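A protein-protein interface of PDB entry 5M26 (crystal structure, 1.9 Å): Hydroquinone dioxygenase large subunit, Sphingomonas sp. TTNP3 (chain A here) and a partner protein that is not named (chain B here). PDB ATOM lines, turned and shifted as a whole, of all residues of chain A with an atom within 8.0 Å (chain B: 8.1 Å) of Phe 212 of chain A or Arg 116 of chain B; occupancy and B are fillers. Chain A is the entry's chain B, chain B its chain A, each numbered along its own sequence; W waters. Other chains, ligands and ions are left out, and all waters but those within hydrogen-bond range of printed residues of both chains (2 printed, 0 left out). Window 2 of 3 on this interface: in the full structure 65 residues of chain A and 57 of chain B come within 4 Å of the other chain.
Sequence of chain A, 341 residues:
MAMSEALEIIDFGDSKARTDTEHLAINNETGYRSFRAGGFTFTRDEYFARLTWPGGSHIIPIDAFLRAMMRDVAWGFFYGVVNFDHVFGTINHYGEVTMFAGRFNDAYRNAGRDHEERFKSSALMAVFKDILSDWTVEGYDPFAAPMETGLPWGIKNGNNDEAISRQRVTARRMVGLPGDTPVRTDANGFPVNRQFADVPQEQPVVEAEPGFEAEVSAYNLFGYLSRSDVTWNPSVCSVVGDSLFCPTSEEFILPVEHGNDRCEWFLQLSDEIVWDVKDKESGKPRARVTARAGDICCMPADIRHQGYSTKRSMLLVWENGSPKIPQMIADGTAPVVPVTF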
ATOM      1  N   VAL A 206      39.389   1.720 -16.954  1.00  0.00           N
ATOM      2  CA  VAL A 206      38.328   2.555 -17.450  1.00  0.00           C
ATOM      3  C   VAL A 206      37.625   1.739 -18.534  1.00  0.00           C
ATOM      4  O   VAL A 206      38.241   1.396 -19.544  1.00  0.00           O
ATOM      5  CB  VAL A 206      38.869   3.872 -18.039  1.00  0.00           C
ATOM      6  CG1 VAL A 206      37.730   4.719 -18.581  1.00  0.00           C
ATOM      7  CG2 VAL A 206      39.671   4.662 -17.013  1.00  0.00           C
ATOM      8  N   GLU A 207      36.353   1.391 -18.306  1.00  0.00           N
ATOM      9  CA  GLU A 207      35.553   0.800 -19.362  1.00  0.00           C
ATOM     10  C   GLU A 207      34.267   1.567 -19.610  1.00  0.00           C
ATOM     11  O   GLU A 207      33.367   1.595 -18.771  1.00  0.00           O
ATOM     12  CB  GLU A 207      35.327  -0.707 -19.170  1.00  0.00           C
ATOM     13  CG  GLU A 207      35.094  -1.180 -17.763  1.00  0.00           C
ATOM     14  CD  GLU A 207      35.914  -2.416 -17.414  1.00  0.00           C
ATOM     15  OE1 GLU A 207      36.983  -2.642 -18.022  1.00  0.00           O
ATOM     16  OE2 GLU A 207      35.508  -3.137 -16.491  1.00  0.00           O
ATOM     17  N   ALA A 208      34.238   2.241 -20.753  1.00  0.00           N
ATOM     18  CA  ALA A 208      33.076   2.963 -21.200  1.00  0.00           C
ATOM     19  C   ALA A 208      32.203   2.012 -21.996  1.00  0.00           C
ATOM     20  O   ALA A 208      32.699   1.121 -22.675  1.00  0.00           O
ATOM     21  CB  ALA A 208      33.474   4.158 -22.053  1.00  0.00           C
ATOM     22  N   GLU A 209      30.901   2.208 -21.889  1.00  0.00           N
ATOM     23  CA  GLU A 209      29.946   1.565 -22.768  1.00  0.00           C
ATOM     24  C   GLU A 209      29.969   2.310 -24.103  1.00  0.00           C
ATOM     25  O   GLU A 209      30.319   3.498 -24.131  1.00  0.00           O
ATOM     26  CB  GLU A 209      28.554   1.624 -22.123  1.00  0.00           C
ATOM     27  CG  GLU A 209      28.443   0.762 -20.881  1.00  0.00           C
ATOM     28  CD  GLU A 209      28.568  -0.726 -21.198  1.00  0.00           C
ATOM     29  OE1 GLU A 209      27.814  -1.226 -22.058  1.00  0.00           O
ATOM     30  OE2 GLU A 209      29.420  -1.407 -20.590  1.00  0.00           O
ATOM     31  N   PRO A 210      29.600   1.635 -25.217  1.00  0.00           N
ATOM     32  CA  PRO A 210      29.628   2.315 -26.524  1.00  0.00           C
ATOM     33  C   PRO A 210      28.876   3.651 -26.515  1.00  0.00           C
ATOM     34  O   PRO A 210      27.773   3.739 -25.965  1.00  0.00           O
ATOM     35  CB  PRO A 210      28.932   1.314 -27.453  1.00  0.00           C
ATOM     36  CG  PRO A 210      29.216  -0.011 -26.823  1.00  0.00           C
ATOM     37  CD  PRO A 210      29.086   0.260 -25.344  1.00  0.00           C
ATOM     38  N   GLY A 211      29.486   4.684 -27.090  1.00  0.00           N
ATOM     39  CA  GLY A 211      28.867   6.006 -27.133  1.00  0.00           C
ATOM     40  C   GLY A 211      29.226   6.912 -25.970  1.00  0.00           C
ATOM     41  O   GLY A 211      28.966   8.114 -26.010  1.00  0.00           O
ATOM     42  N   PHE A 212      29.824   6.354 -24.925  1.00  0.00           N
ATOM     43  CA  PHE A 212      30.172   7.163 -23.765  1.00  0.00           C
ATOM     44  C   PHE A 212      31.676   7.304 -23.501  1.00  0.00           C
ATOM     45  O   PHE A 212      32.078   7.753 -22.424  1.00  0.00           O
ATOM     46  CB  PHE A 212      29.474   6.605 -22.520  1.00  0.00           C
ATOM     47  CG  PHE A 212      27.980   6.696 -22.575  1.00  0.00           C
ATOM     48  CD1 PHE A 212      27.343   7.934 -22.451  1.00  0.00           C
ATOM     49  CD2 PHE A 212      27.205   5.548 -22.748  1.00  0.00           C
ATOM     50  CE1 PHE A 212      25.959   8.022 -22.493  1.00  0.00           C
ATOM     51  CE2 PHE A 212      25.822   5.633 -22.799  1.00  0.00           C
ATOM     52  CZ  PHE A 212      25.198   6.870 -22.672  1.00  0.00           C
ATOM     53  N   GLU A 213      32.509   6.959 -24.472  1.00  0.00           N
ATOM     54  CA  GLU A 213      33.957   6.982 -24.229  1.00  0.00           C
ATOM     55  C   GLU A 213      34.520   8.359 -23.888  1.00  0.00           C
ATOM     56  O   GLU A 213      35.500   8.443 -23.160  1.00  0.00           O
ATOM     57  CB  GLU A 213      34.784   6.237 -25.299  1.00  0.00           C
ATOM     58  CG  GLU A 213      34.282   6.272 -26.723  1.00  0.00           C
ATOM     59  CD  GLU A 213      32.981   5.509 -26.939  1.00  0.00           C
ATOM     60  OE1 GLU A 213      31.959   6.186 -27.155  1.00  0.00           O
ATOM     61  OE2 GLU A 213      32.977   4.254 -26.911  1.00  0.00           O
ATOM     62  N   ALA A 214      33.883   9.424 -24.371  1.00  0.00           N
ATOM     63  CA  ALA A 214      34.321  10.792 -24.070  1.00  0.00           C
ATOM     64  C   ALA A 214      34.088  11.241 -22.632  1.00  0.00           C
ATOM     65  O   ALA A 214      34.737  12.192 -22.184  1.00  0.00           O
ATOM     66  CB  ALA A 214      33.660  11.788 -25.009  1.00  0.00           C
ATOM     67  N   GLU A 215      33.161  10.606 -21.906  1.00  0.00           N
ATOM     68  CA  GLU A 215      32.844  11.085 -20.544  1.00  0.00           C
ATOM     69  C   GLU A 215      33.041  10.097 -19.399  1.00  0.00           C
ATOM     70  O   GLU A 215      32.648  10.357 -18.268  1.00  0.00           O
ATOM     71  CB  GLU A 215      31.464  11.741 -20.488  1.00  0.00           C
ATOM     72  CG  GLU A 215      31.521  13.200 -20.934  1.00  0.00           C
ATOM     73  CD  GLU A 215      30.329  14.026 -20.492  1.00  0.00           C
ATOM     74  OE1 GLU A 215      29.239  13.458 -20.188  1.00  0.00           O
ATOM     75  OE2 GLU A 215      30.491  15.266 -20.455  1.00  0.00           O
ATOM     76  N   VAL A 216      33.651   8.963 -19.705  1.00  0.00           N
ATOM     77  CA  VAL A 216      34.080   8.017 -18.699  1.00  0.00           C
ATOM     78  C   VAL A 216      35.594   8.160 -18.752  1.00  0.00           C
ATOM     79  O   VAL A 216      36.239   7.638 -19.658  1.00  0.00           O
ATOM     80  CB  VAL A 216      33.617   6.593 -19.032  1.00  0.00           C
ATOM     81  CG1 VAL A 216      34.040   5.610 -17.937  1.00  0.00           C
ATOM     82  CG2 VAL A 216      32.104   6.570 -19.203  1.00  0.00           C
ATOM     83  N   SER A 217      36.161   8.879 -17.789  1.00  0.00           N
ATOM     84  CA  SER A 217      37.562   9.248 -17.881  1.00  0.00           C
ATOM     85  C   SER A 217      38.241   9.258 -16.507  1.00  0.00           C
ATOM     86  O   SER A 217      37.699   9.780 -15.529  1.00  0.00           O
ATOM     87  CB  SER A 217      37.695  10.600 -18.560  1.00  0.00           C
ATOM     88  OG  SER A 217      39.050  10.879 -18.870  1.00  0.00           O
ATOM     89  N   TRP B  68      23.268   6.189  -4.831  1.00  0.00           N
ATOM     90  CA  TRP B  68      23.563   6.979  -6.019  1.00  0.00           C
ATOM     91  C   TRP B  68      23.685   8.462  -5.693  1.00  0.00           C
ATOM     92  O   TRP B  68      22.978   8.966  -4.831  1.00  0.00           O
ATOM     93  CB  TRP B  68      22.482   6.735  -7.080  1.00  0.00           C
ATOM     94  CG  TRP B  68      22.572   5.375  -7.656  1.00  0.00           C
ATOM     95  CD1 TRP B  68      21.909   4.257  -7.233  1.00  0.00           C
ATOM     96  CD2 TRP B  68      23.377   4.971  -8.765  1.00  0.00           C
ATOM     97  NE1 TRP B  68      22.259   3.159  -8.010  1.00  0.00           N
ATOM     98  CE2 TRP B  68      23.166   3.572  -8.954  1.00  0.00           C
ATOM     99  CE3 TRP B  68      24.284   5.640  -9.597  1.00  0.00           C
ATOM    100  CZ2 TRP B  68      23.814   2.846  -9.957  1.00  0.00           C
ATOM    101  CZ3 TRP B  68      24.932   4.910 -10.606  1.00  0.00           C
ATOM    102  CH2 TRP B  68      24.696   3.530 -10.771  1.00  0.00           C
ATOM    103  N   LEU B  88      28.910   4.637 -13.405  1.00  0.00           N
ATOM    104  CA  LEU B  88      28.350   5.852 -13.966  1.00  0.00           C
ATOM    105  C   LEU B  88      27.163   5.476 -14.807  1.00  0.00           C
ATOM    106  O   LEU B  88      27.213   4.498 -15.560  1.00  0.00           O
ATOM    107  CB  LEU B  88      29.366   6.585 -14.864  1.00  0.00           C
ATOM    108  CG  LEU B  88      30.573   7.221 -14.173  1.00  0.00           C
ATOM    109  CD1 LEU B  88      31.565   7.768 -15.200  1.00  0.00           C
ATOM    110  CD2 LEU B  88      30.100   8.311 -13.214  1.00  0.00           C
ATOM    111  N   LEU B  89      26.125   6.302 -14.705  1.00  0.00           N
ATOM    112  CA  LEU B  89      24.848   6.049 -15.339  1.00  0.00           C
ATOM    113  C   LEU B  89      24.350   7.369 -15.911  1.00  0.00           C
ATOM    114  O   LEU B  89      24.300   8.367 -15.202  1.00  0.00           O
ATOM    115  CB  LEU B  89      23.880   5.509 -14.278  1.00  0.00           C
ATOM    116  CG  LEU B  89      22.478   5.042 -14.632  1.00  0.00           C
ATOM    117  CD1 LEU B  89      22.059   4.010 -13.603  1.00  0.00           C
ATOM    118  CD2 LEU B  89      21.543   6.224 -14.532  1.00  0.00           C
ATOM    119  N   LYS B  90      24.008   7.382 -17.200  1.00  0.00           N
ATOM    120  CA  LYS B  90      23.481   8.572 -17.838  1.00  0.00           C
ATOM    121  C   LYS B  90      21.982   8.680 -17.527  1.00  0.00           C
ATOM    122  O   LYS B  90      21.186   7.876 -18.001  1.00  0.00           O
ATOM    123  CB  LYS B  90      23.701   8.495 -19.353  1.00  0.00           C
ATOM    124  CG  LYS B  90      23.232   9.730 -20.098  1.00  0.00           C
ATOM    125  CD  LYS B  90      24.420  10.612 -20.429  1.00  0.00           C
ATOM    126  CE  LYS B  90      24.077  12.086 -20.367  1.00  0.00           C
ATOM    127  NZ  LYS B  90      25.280  12.836 -20.828  1.00  0.00           N
ATOM    128  N   LEU B  91      21.584   9.670 -16.743  1.00  0.00           N
ATOM    129  CA  LEU B  91      20.170   9.752 -16.318  1.00  0.00           C
ATOM    130  C   LEU B  91      19.262  10.119 -17.493  1.00  0.00           C
ATOM    131  O   LEU B  91      19.603  11.005 -18.276  1.00  0.00           O
ATOM    132  CB  LEU B  91      19.983  10.745 -15.165  1.00  0.00           C
ATOM    133  CG  LEU B  91      20.634  10.437 -13.815  1.00  0.00           C
ATOM    134  CD1 LEU B  91      20.761  11.706 -12.975  1.00  0.00           C
ATOM    135  CD2 LEU B  91      19.796   9.393 -13.084  1.00  0.00           C
ATOM    136  N   ASP B  92      18.128   9.415 -17.624  1.00  0.00           N
ATOM    137  CA  ASP B  92      17.149   9.735 -18.664  1.00  0.00           C
ATOM    138  C   ASP B  92      16.623  11.141 -18.444  1.00  0.00           C
ATOM    139  O   ASP B  92      16.499  11.892 -19.396  1.00  0.00           O
ATOM    140  CB  ASP B  92      15.966   8.762 -18.656  1.00  0.00           C
ATOM    141  CG  ASP B  92      16.326   7.408 -19.189  1.00  0.00           C
ATOM    142  OD1 ASP B  92      17.373   7.287 -19.859  1.00  0.00           O
ATOM    143  OD2 ASP B  92      15.561   6.457 -18.942  1.00  0.00           O
ATOM    144  N   ASN B  93      16.324  11.477 -17.190  1.00  0.00           N
ATOM    145  CA  ASN B  93      15.845  12.796 -16.789  1.00  0.00           C
ATOM    146  C   ASN B  93      16.574  13.247 -15.516  1.00  0.00           C
ATOM    147  O   ASN B  93      16.105  12.993 -14.399  1.00  0.00           O
ATOM    148  CB  ASN B  93      14.341  12.740 -16.496  1.00  0.00           C
ATOM    149  CG  ASN B  93      13.516  12.463 -17.741  1.00  0.00           C
ATOM    150  OD1 ASN B  93      13.204  13.374 -18.502  1.00  0.00           O
ATOM    151  ND2 ASN B  93      13.168  11.200 -17.954  1.00  0.00           N
ATOM    152  N   PRO B 113      18.458   4.492 -10.392  1.00  0.00           N
ATOM    153  CA  PRO B 113      17.790   5.537 -11.160  1.00  0.00           C
ATOM    154  C   PRO B 113      17.613   5.090 -12.593  1.00  0.00           C
ATOM    155  O   PRO B 113      18.288   4.157 -13.034  1.00  0.00           O
ATOM    156  CB  PRO B 113      18.783   6.715 -11.123  1.00  0.00           C
ATOM    157  CG  PRO B 113      19.778   6.373 -10.083  1.00  0.00           C
ATOM    158  CD  PRO B 113      19.838   4.882 -10.042  1.00  0.00           C
ATOM    159  N   GLU B 114      16.734   5.785 -13.307  1.00  0.00           N
ATOM    160  CA  GLU B 114      16.432   5.501 -14.708  1.00  0.00           C
ATOM    161  C   GLU B 114      17.469   6.123 -15.620  1.00  0.00           C
ATOM    162  O   GLU B 114      17.654   7.335 -15.618  1.00  0.00           O
ATOM    163  CB  GLU B 114      15.060   6.054 -15.086  1.00  0.00           C
ATOM    164  CG  GLU B 114      13.893   5.373 -14.399  1.00  0.00           C
ATOM    165  CD  GLU B 114      14.001   3.862 -14.420  1.00  0.00           C
ATOM    166  OE1 GLU B 114      14.284   3.276 -15.486  1.00  0.00           O
ATOM    167  OE2 GLU B 114      13.824   3.260 -13.345  1.00  0.00           O
ATOM    168  N   GLY B 115      18.152   5.298 -16.397  1.00  0.00           N
ATOM    169  CA  GLY B 115      19.153   5.825 -17.325  1.00  0.00           C
ATOM    170  C   GLY B 115      19.917   4.716 -17.998  1.00  0.00           C
ATOM    171  O   GLY B 115      19.604   3.565 -17.795  1.00  0.00           O
ATOM    172  N   ARG B 116      20.920   5.069 -18.799  1.00  0.00           N
ATOM    173  CA  ARG B 116      21.723   4.072 -19.515  1.00  0.00           C
ATOM    174  C   ARG B 116      23.086   3.937 -18.849  1.00  0.00           C
ATOM    175  O   ARG B 116      23.646   4.931 -18.392  1.00  0.00           O
ATOM    176  CB  ARG B 116      21.885   4.464 -20.980  1.00  0.00           C
ATOM    177  CG  ARG B 116      20.563   4.666 -21.707  1.00  0.00           C
ATOM    178  CD  ARG B 116      20.773   4.993 -23.179  1.00  0.00           C
ATOM    179  NE  ARG B 116      21.683   6.118 -23.402  1.00  0.00           N
ATOM    180  CZ  ARG B 116      21.317   7.404 -23.424  1.00  0.00           C
ATOM    181  NH1 ARG B 116      22.215   8.355 -23.649  1.00  0.00           N
ATOM    182  NH2 ARG B 116      20.048   7.747 -23.219  1.00  0.00           N
ATOM    183  N   LYS B 117      23.599   2.708 -18.789  1.00  0.00           N
ATOM    184  CA  LYS B 117      24.913   2.439 -18.222  1.00  0.00           C
ATOM    185  C   LYS B 117      25.990   3.182 -19.038  1.00  0.00           C
ATOM    186  O   LYS B 117      26.077   3.027 -20.258  1.00  0.00           O
ATOM    187  CB  LYS B 117      25.195   0.932 -18.186  1.00  0.00           C
ATOM    188  CG  LYS B 117      26.489   0.585 -17.468  1.00  0.00           C
ATOM    189  CD  LYS B 117      26.881  -0.887 -17.598  1.00  0.00           C
ATOM    190  CE  LYS B 117      28.301  -1.108 -17.075  1.00  0.00           C
ATOM    191  NZ  LYS B 117      28.642  -2.546 -16.867  1.00  0.00           N
ATOM    192  N   MET B 118      26.799   3.990 -18.359  1.00  0.00           N
ATOM    193  CA  MET B 118      27.854   4.753 -19.049  1.00  0.00           C
ATOM    194  C   MET B 118      29.191   4.044 -19.012  1.00  0.00           C
ATOM    195  O   MET B 118      29.935   4.042 -19.994  1.00  0.00           O
ATOM    196  CB  MET B 118      28.041   6.117 -18.414  1.00  0.00           C
ATOM    197  CG  MET B 118      27.032   7.143 -18.853  1.00  0.00           C
ATOM    198  SD  MET B 118      27.279   8.637 -17.895  1.00  0.00           S
ATOM    199  CE  MET B 118      28.685   9.388 -18.735  1.00  0.00           C
ATOM    200  N   GLY B 119      29.516   3.503 -17.846  1.00  0.00           N
ATOM    201  CA  GLY B 119      30.747   2.783 -17.693  1.00  0.00           C
ATOM    202  C   GLY B 119      31.111   2.470 -16.267  1.00  0.00           C
ATOM    203  O   GLY B 119      30.342   2.673 -15.332  1.00  0.00           O
ATOM    204  N   PRO B 132      30.860  13.470 -14.334  1.00  0.00           N
ATOM    205  CA  PRO B 132      30.332  14.493 -15.240  1.00  0.00           C
ATOM    206  C   PRO B 132      28.902  14.880 -14.915  1.00  0.00           C
ATOM    207  O   PRO B 132      28.082  14.006 -14.535  1.00  0.00           O
ATOM    208  CB  PRO B 132      30.375  13.813 -16.613  1.00  0.00           C
ATOM    209  CG  PRO B 132      30.275  12.353 -16.325  1.00  0.00           C
ATOM    210  CD  PRO B 132      30.973  12.146 -14.987  1.00  0.00           C
ATOM    211  N   GLY B 134      25.198  15.316 -15.236  1.00  0.00           N
ATOM    212  CA  GLY B 134      24.182  14.634 -16.037  1.00  0.00           C
ATOM    213  C   GLY B 134      24.219  13.144 -15.768  1.00  0.00           C
ATOM    214  O   GLY B 134      23.307  12.383 -16.157  1.00  0.00           O
ATOM    215  N   ALA B 135      25.287  12.721 -15.105  1.00  0.00           N
ATOM    216  CA  ALA B 135      25.450  11.336 -14.774  1.00  0.00           C
ATOM    217  C   ALA B 135      25.089  11.135 -13.309  1.00  0.00           C
ATOM    218  O   ALA B 135      25.175  12.069 -12.498  1.00  0.00           O
ATOM    219  CB  ALA B 135      26.877  10.884 -15.049  1.00  0.00           C
ATOM    220  N   ALA B 136      24.636   9.925 -12.990  1.00  0.00           N
ATOM    221  CA  ALA B 136      24.549   9.492 -11.595  1.00  0.00           C
ATOM    222  C   ALA B 136      25.759   8.630 -11.366  1.00  0.00           C
ATOM    223  O   ALA B 136      26.222   7.941 -12.286  1.00  0.00           O
ATOM    224  CB  ALA B 136      23.281   8.688 -11.347  1.00  0.00           C
HETATM  225  O   HOH W   1      31.126  -0.536 -18.265  1.00  0.00           O
HETATM  226  O   HOH W   2      26.724  13.308 -18.536  1.00  0.00           O
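NZ of Lys 117 of chain B lies within salt-bridge range of OE2 of Glu 209 of chain A, at 3.97 Å.
The backbone NH of Glu 209 of chain A lies within hydrogen-bond range of the backbone carbonyl oxygen of Met 118 of chain B, at 2.8 Å.
O of Glu 207 of chain A touches CA of Gly 119 of chain B, at 3.1 Å.
O of Met 118 of chain B touches CA of Ala 208 of chain A, at 3.5 Å.
Phe 212 of chain A touches Lys 90 of chain B.
CZ of Phe 212 of chain A touches NH1 of Arg 116 of chain B, 3.5 Å away.
CE2 of Phe 212 of chain A touches O of Lys 117 of chain B, at 3.6 Å.
Phe 212 of chain A touches Met 118 of chain B (CB to O, 3.6 Å).
Glu 215 of chain A touches Pro 132 of chain B (O to CG, 3.7 Å).
Met 118 of chain B touches Val 216 of chain A (O to CG2, 3.4 Å).
Of the 12 printed residues of chain A, 6 touch a printed residue of chain B.
Hydrophobic or aromatic side chains of chain A within 4 Å of the printed part of chain B: Phe 212 and Val 216.
Of the 18 printed residues of chain B, 6 touch a printed residue of chain A.
Hydrophobic or aromatic side chains of chain B that line the printed part of chain A: Met 118 and Pro 132.
Among the printed residues, 10 pairs touch across the chains.
Among the printed residues, Asp or Glu carboxylates within 4 Å of a Lys or Arg side-chain nitrogen of the other chain: Glu 209 of chain A with Lys 117 of chain B.
The backbone NH (N) of Met 118 of chain B sits at hydrogen-bond distance from the backbone carbonyl oxygen (O) of Leu 88 of chain B (2.9 Å).
The backbone carbonyl oxygen (O) of Gly 119 of chain B is in hydrogen-bond range of the backbone NH (N) of Leu 88 of chain B (3.1 Å).
The backbone carbonyl oxygen (O) of Arg 116 of chain B is in hydrogen-bond range of the backbone NH (N) of Lys 90 of chain B (2.7 Å).
SD of Met 118 of chain B sits close to N of Lys 90 of chain B (3.6 Å).
Of the printed residues of chain B, Glu 207 of chain A touches Gly 119 (3.1 Å).
Pro 210 of chain A touches none of the printed residues of chain B.
Phe 212 of chain A touches just these residues of chain B: Lys 90, Arg 116, Lys 117 and Met 118.
No residue of chain A comes within 4 Å of Gly 115 of chain B.
Arg 116 of chain B touches just one residue of chain A: Phe 212 (3.5 Å).
Printed residues of chain A within 4 Å of Gly 119 of chain B: Glu 207 (3.1 Å).
The nearest printed residue of chain B that does not touch Glu 207 of chain A is Met 118 of chain B (4.4 Å).
Water W2 bridges the side-chain amino group of Lys 90 of chain B (2.7 Å) and the side-chain carboxylate of Glu 215 of chain A (3.0 Å).
Water W1 lies within hydrogen-bond range of the side-chain carboxylate of Glu 209 of chain A (3.0 Å), the backbone carbonyl oxygen of Glu 207 of chain A (3.1 Å) and the side-chain amino group of Lys 117 of chain B (3.5 Å).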
